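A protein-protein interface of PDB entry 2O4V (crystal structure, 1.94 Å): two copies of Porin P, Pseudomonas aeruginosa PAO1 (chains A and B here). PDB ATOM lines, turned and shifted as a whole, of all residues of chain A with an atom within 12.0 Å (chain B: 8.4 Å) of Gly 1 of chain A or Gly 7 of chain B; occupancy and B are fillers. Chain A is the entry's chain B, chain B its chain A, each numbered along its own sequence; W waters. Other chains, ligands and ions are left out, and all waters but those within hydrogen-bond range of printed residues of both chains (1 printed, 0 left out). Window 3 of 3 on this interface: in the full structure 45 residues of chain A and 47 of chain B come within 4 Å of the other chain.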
ATOM      1  N   GLY A   1      17.644 -16.366  16.485  1.00  0.00           N
ATOM      2  CA  GLY A   1      17.909 -15.504  15.301  1.00  0.00           C
ATOM      3  C   GLY A   1      18.136 -14.046  15.648  1.00  0.00           C
ATOM      4  O   GLY A   1      17.952 -13.623  16.794  1.00  0.00           O
ATOM      5  N   THR A   2      18.521 -13.266  14.645  1.00  0.00           N
ATOM      6  CA  THR A   2      18.819 -11.856  14.856  1.00  0.00           C
ATOM      7  C   THR A   2      17.557 -10.994  14.808  1.00  0.00           C
ATOM      8  O   THR A   2      16.513 -11.401  14.278  1.00  0.00           O
ATOM      9  CB  THR A   2      19.862 -11.323  13.834  1.00  0.00           C
ATOM     10  OG1 THR A   2      19.321 -11.400  12.511  1.00  0.00           O
ATOM     11  CG2 THR A   2      21.183 -12.123  13.906  1.00  0.00           C
ATOM     12  N   VAL A   3      17.646  -9.808  15.397  1.00  0.00           N
ATOM     13  CA  VAL A   3      16.603  -8.799  15.241  1.00  0.00           C
ATOM     14  C   VAL A   3      17.288  -7.519  14.786  1.00  0.00           C
ATOM     15  O   VAL A   3      18.187  -6.997  15.468  1.00  0.00           O
ATOM     16  CB  VAL A   3      15.808  -8.564  16.539  1.00  0.00           C
ATOM     17  CG1 VAL A   3      14.732  -7.505  16.318  1.00  0.00           C
ATOM     18  CG2 VAL A   3      15.203  -9.867  17.034  1.00  0.00           C
ATOM     19  N   THR A   4      16.886  -7.049  13.610  1.00  0.00           N
ATOM     20  CA  THR A   4      17.486  -5.872  12.990  1.00  0.00           C
ATOM     21  C   THR A   4      16.400  -4.951  12.432  1.00  0.00           C
ATOM     22  O   THR A   4      15.209  -5.280  12.461  1.00  0.00           O
ATOM     23  CB  THR A   4      18.476  -6.253  11.854  1.00  0.00           C
ATOM     24  OG1 THR A   4      17.794  -7.013  10.847  1.00  0.00           O
ATOM     25  CG2 THR A   4      19.655  -7.063  12.389  1.00  0.00           C
ATOM     26  N   THR A   5      16.822  -3.788  11.947  1.00  0.00           N
ATOM     27  CA  THR A   5      15.926  -2.863  11.272  1.00  0.00           C
ATOM     28  C   THR A   5      16.613  -2.325  10.025  1.00  0.00           C
ATOM     29  O   THR A   5      17.839  -2.299   9.956  1.00  0.00           O
ATOM     30  CB  THR A   5      15.469  -1.711  12.208  1.00  0.00           C
ATOM     31  OG1 THR A   5      14.513  -0.895  11.522  1.00  0.00           O
ATOM     32  CG2 THR A   5      16.652  -0.854  12.679  1.00  0.00           C
ATOM     33  N   ILE A  12      14.034  -0.787  21.975  1.00  0.00           N
ATOM     34  CA  ILE A  12      12.734  -1.271  22.442  1.00  0.00           C
ATOM     35  C   ILE A  12      12.702  -1.395  23.962  1.00  0.00           C
ATOM     36  O   ILE A  12      13.735  -1.600  24.607  1.00  0.00           O
ATOM     37  CB  ILE A  12      12.277  -2.580  21.742  1.00  0.00           C
ATOM     38  CG1 ILE A  12      13.183  -3.758  22.097  1.00  0.00           C
ATOM     39  CG2 ILE A  12      12.233  -2.392  20.218  1.00  0.00           C
ATOM     40  CD1 ILE A  12      12.617  -5.115  21.640  1.00  0.00           C
ATOM     41  N   VAL B   3      18.463  -7.709  21.811  1.00  0.00           N
ATOM     42  CA  VAL B   3      17.131  -8.097  21.355  1.00  0.00           C
ATOM     43  C   VAL B   3      17.332  -9.232  20.367  1.00  0.00           C
ATOM     44  O   VAL B   3      17.988  -9.056  19.331  1.00  0.00           O
ATOM     45  CB  VAL B   3      16.373  -6.933  20.691  1.00  0.00           C
ATOM     46  CG1 VAL B   3      14.991  -7.411  20.163  1.00  0.00           C
ATOM     47  CG2 VAL B   3      16.223  -5.762  21.668  1.00  0.00           C
ATOM     48  N   THR B   4      16.827 -10.409  20.725  1.00  0.00           N
ATOM     49  CA  THR B   4      16.954 -11.599  19.882  1.00  0.00           C
ATOM     50  C   THR B   4      15.592 -12.264  19.692  1.00  0.00           C
ATOM     51  O   THR B   4      14.577 -11.797  20.222  1.00  0.00           O
ATOM     52  CB  THR B   4      17.978 -12.632  20.442  1.00  0.00           C
ATOM     53  OG1 THR B   4      17.532 -13.137  21.706  1.00  0.00           O
ATOM     54  CG2 THR B   4      19.386 -12.026  20.588  1.00  0.00           C
ATOM     55  N   THR B   5      15.582 -13.340  18.912  1.00  0.00           N
ATOM     56  CA  THR B   5      14.384 -14.145  18.693  1.00  0.00           C
ATOM     57  C   THR B   5      14.771 -15.626  18.650  1.00  0.00           C
ATOM     58  O   THR B   5      15.922 -15.961  18.358  1.00  0.00           O
ATOM     59  CB  THR B   5      13.603 -13.700  17.422  1.00  0.00           C
ATOM     60  OG1 THR B   5      12.386 -14.448  17.323  1.00  0.00           O
ATOM     61  CG2 THR B   5      14.419 -13.894  16.160  1.00  0.00           C
ATOM     62  N   ASP B   6      13.834 -16.513  18.973  1.00  0.00           N
ATOM     63  CA  ASP B   6      14.153 -17.949  18.977  1.00  0.00           C
ATOM     64  C   ASP B   6      13.808 -18.652  17.661  1.00  0.00           C
ATOM     65  O   ASP B   6      14.164 -19.810  17.459  1.00  0.00           O
ATOM     66  CB  ASP B   6      13.524 -18.670  20.184  1.00  0.00           C
ATOM     67  CG  ASP B   6      12.010 -18.558  20.222  1.00  0.00           C
ATOM     68  OD1 ASP B   6      11.453 -17.583  19.668  1.00  0.00           O
ATOM     69  OD2 ASP B   6      11.370 -19.450  20.825  1.00  0.00           O
ATOM     70  N   GLY B   7      13.120 -17.943  16.772  1.00  0.00           N
ATOM     71  CA  GLY B   7      12.784 -18.474  15.456  1.00  0.00           C
ATOM     72  C   GLY B   7      13.681 -17.866  14.398  1.00  0.00           C
ATOM     73  O   GLY B   7      14.843 -17.541  14.670  1.00  0.00           O
ATOM     74  N   ALA B   8      13.138 -17.708  13.191  1.00  0.00           N
ATOM     75  CA  ALA B   8      13.857 -17.087  12.080  1.00  0.00           C
ATOM     76  C   ALA B   8      14.170 -15.613  12.378  1.00  0.00           C
ATOM     77  O   ALA B   8      13.457 -14.966  13.160  1.00  0.00           O
ATOM     78  CB  ALA B   8      13.030 -17.208  10.801  1.00  0.00           C
ATOM     79  N   ASP B   9      15.224 -15.094  11.749  1.00  0.00           N
ATOM     80  CA  ASP B   9      15.616 -13.681  11.856  1.00  0.00           C
ATOM     81  C   ASP B   9      14.431 -12.755  11.625  1.00  0.00           C
ATOM     82  O   ASP B   9      13.559 -13.040  10.799  1.00  0.00           O
ATOM     83  CB  ASP B   9      16.726 -13.337  10.847  1.00  0.00           C
ATOM     84  CG  ASP B   9      18.003 -14.135  11.071  1.00  0.00           C
ATOM     85  OD1 ASP B   9      18.239 -14.602  12.207  1.00  0.00           O
ATOM     86  OD2 ASP B   9      18.787 -14.287  10.106  1.00  0.00           O
ATOM     87  N   ILE B  10      14.412 -11.644  12.352  1.00  0.00           N
ATOM     88  CA  ILE B  10      13.294 -10.705  12.297  1.00  0.00           C
ATOM     89  C   ILE B  10      13.767  -9.295  11.943  1.00  0.00           C
ATOM     90  O   ILE B  10      14.812  -8.840  12.419  1.00  0.00           O
ATOM     91  CB  ILE B  10      12.502 -10.688  13.639  1.00  0.00           C
ATOM     92  CG1 ILE B  10      11.521 -11.872  13.705  1.00  0.00           C
ATOM     93  CG2 ILE B  10      11.755  -9.368  13.819  1.00  0.00           C
ATOM     94  CD1 ILE B  10      10.749 -11.997  15.026  1.00  0.00           C
ATOM     95  N   THR B  22       9.476 -11.959   9.926  1.00  0.00           N
ATOM     96  CA  THR B  22      10.588 -12.889   9.725  1.00  0.00           C
ATOM     97  C   THR B  22      11.084 -12.768   8.286  1.00  0.00           C
ATOM     98  O   THR B  22      10.287 -12.559   7.361  1.00  0.00           O
ATOM     99  CB  THR B  22      10.222 -14.366  10.061  1.00  0.00           C
ATOM    100  OG1 THR B  22       9.146 -14.810   9.226  1.00  0.00           O
ATOM    101  CG2 THR B  22       9.810 -14.509  11.522  1.00  0.00           C
ATOM    102  N   THR B  23      12.400 -12.897   8.098  1.00  0.00           N
ATOM    103  CA  THR B  23      13.015 -12.639   6.795  1.00  0.00           C
ATOM    104  C   THR B  23      12.753 -13.748   5.773  1.00  0.00           C
ATOM    105  O   THR B  23      13.022 -13.579   4.580  1.00  0.00           O
ATOM    106  CB  THR B  23      14.540 -12.371   6.913  1.00  0.00           C
ATOM    107  OG1 THR B  23      15.197 -13.539   7.421  1.00  0.00           O
ATOM    108  CG2 THR B  23      14.810 -11.182   7.833  1.00  0.00           C
ATOM    109  N   ASP B  24      12.232 -14.880   6.244  1.00  0.00           N
ATOM    110  CA  ASP B  24      11.873 -15.987   5.358  1.00  0.00           C
ATOM    111  C   ASP B  24      10.452 -15.852   4.800  1.00  0.00           C
ATOM    112  O   ASP B  24       9.975 -16.737   4.083  1.00  0.00           O
ATOM    113  CB  ASP B  24      12.051 -17.329   6.071  1.00  0.00           C
ATOM    114  CG  ASP B  24      11.220 -17.448   7.342  1.00  0.00           C
ATOM    115  OD1 ASP B  24      10.396 -16.555   7.654  1.00  0.00           O
ATOM    116  OD2 ASP B  24      11.395 -18.460   8.042  1.00  0.00           O
ATOM    117  N   PHE B  27       6.240 -15.394   8.726  1.00  0.00           N
ATOM    118  CA  PHE B  27       5.436 -14.727   9.748  1.00  0.00           C
ATOM    119  C   PHE B  27       5.617 -13.217   9.719  1.00  0.00           C
ATOM    120  O   PHE B  27       6.721 -12.720   9.470  1.00  0.00           O
ATOM    121  CB  PHE B  27       5.783 -15.249  11.148  1.00  0.00           C
ATOM    122  CG  PHE B  27       5.602 -16.734  11.316  1.00  0.00           C
ATOM    123  CD1 PHE B  27       4.330 -17.289  11.429  1.00  0.00           C
ATOM    124  CD2 PHE B  27       6.708 -17.575  11.380  1.00  0.00           C
ATOM    125  CE1 PHE B  27       4.156 -18.660  11.591  1.00  0.00           C
ATOM    126  CE2 PHE B  27       6.546 -18.952  11.539  1.00  0.00           C
ATOM    127  CZ  PHE B  27       5.265 -19.495  11.644  1.00  0.00           C
HETATM  128  O   HOH W   1      17.395  -9.645  11.366  1.00  0.00           O
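Hydrophobic or aromatic side chains of chain B that line the printed part of chain A: Val 3. Of the 6 printed residues of chain A, 5 touch a printed residue of chain B. Printed residues of chain A that touch a printed residue of chain B: Gly 1, Thr 2, Val 3, Thr 4 and Ile 12. Among the printed residues, 13 pairs touch across the chains.
The backbone NH (N) of Thr 23 of chain B is in hydrogen-bond range of the backbone carbonyl oxygen (O) of Asp 9 of chain B (2.9 Å).
Gly 7 of chain B touches just one residue of chain A: Gly 1 (3.5 Å). Of chain B, only Thr 5, Asp 9 and Ile 10 come within 4 Å of Thr 2 of chain A. Printed residues of chain A within 4 Å of Thr 4 of chain B: Gly 1 (3.8 Å) and Val 3 (3.6 Å). Of chain A, only Gly 1 (2.6 Å), Thr 2 (3.8 Å) and Val 3 (3.97 Å) come within 4 Å of Thr 5 of chain B. No residue of chain A comes within 4 Å of Ala 8 of chain B. Asp 9 of chain B touches two residues of chain A. Of the printed residues of chain B, Val 3 of chain A touches Val 3, Thr 4, Thr 5 and Ile 10. Of the printed residues of chain B, Ile 12 of chain A touches Val 3. Phe 27 of chain B touches none of the printed residues of chain A. Thr 23 of chain B touches none of the printed residues of chain A. The nearest residue of chain B that does not touch Gly 1 of chain A is Asp 6 of chain B (4.6 Å). The nearest printed residue of chain A that does not touch Ile 10 of chain B is Thr 5 of chain A (5.5 Å).
N of Gly 1 of chain A is in hydrogen-bond range of O of Thr 5 of chain B (2.6 Å). The side-chain carboxylate (OD1) of Asp 9 of chain B lies within hydrogen-bond range of the backbone NH (N) of Thr 2 of chain A (2.8 Å). The backbone NH of Ile 10 of chain B is in hydrogen-bond range of the backbone carbonyl oxygen of Thr 2 of chain A (2.9 Å). N of Thr 4 of chain A sits at hydrogen-bond distance from O of Ile 10 of chain B, at 3.0 Å.
Water W1 lies within hydrogen-bond range of OG1 of Thr 4 of chain A, OG1 of Thr 2 of chain A and O of Ile 10 of chain B.
Among the printed residues, merely in contact across the chains: Gly 1 of chain A with Thr 4 of chain B, Gly 1 of chain A with Gly 7 of chain B, Gly 1 of chain A with Asp 9 of chain B, Thr 2 of chain A with Thr 5 of chain B, Val 3 of chain A with Val 3 of chain B, Val 3 of chain A with Thr 4 of chain B, Val 3 of chain A with Thr 5 of chain B, Val 3 of chain A with Ile 10 of chain B and Ile 12 of chain A with Val 3 of chain B.
Val 3 of chain A touches its own counterpart, Val 3 of chain B. Val 3 of chain A touches Thr 4 of chain B, but with the chains exchanged Thr 4 of chain A does not touch Val 3 of chain B (6.2 Å). Val 3 of chain A touches Thr 5 of chain B, but with the chains exchanged Thr 5 of chain A does not touch Val 3 of chain B (9.1 Å). Of the 13 pairs that touch across the chains among the printed residues, 1 has its exchanged pair printed and touching as well.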
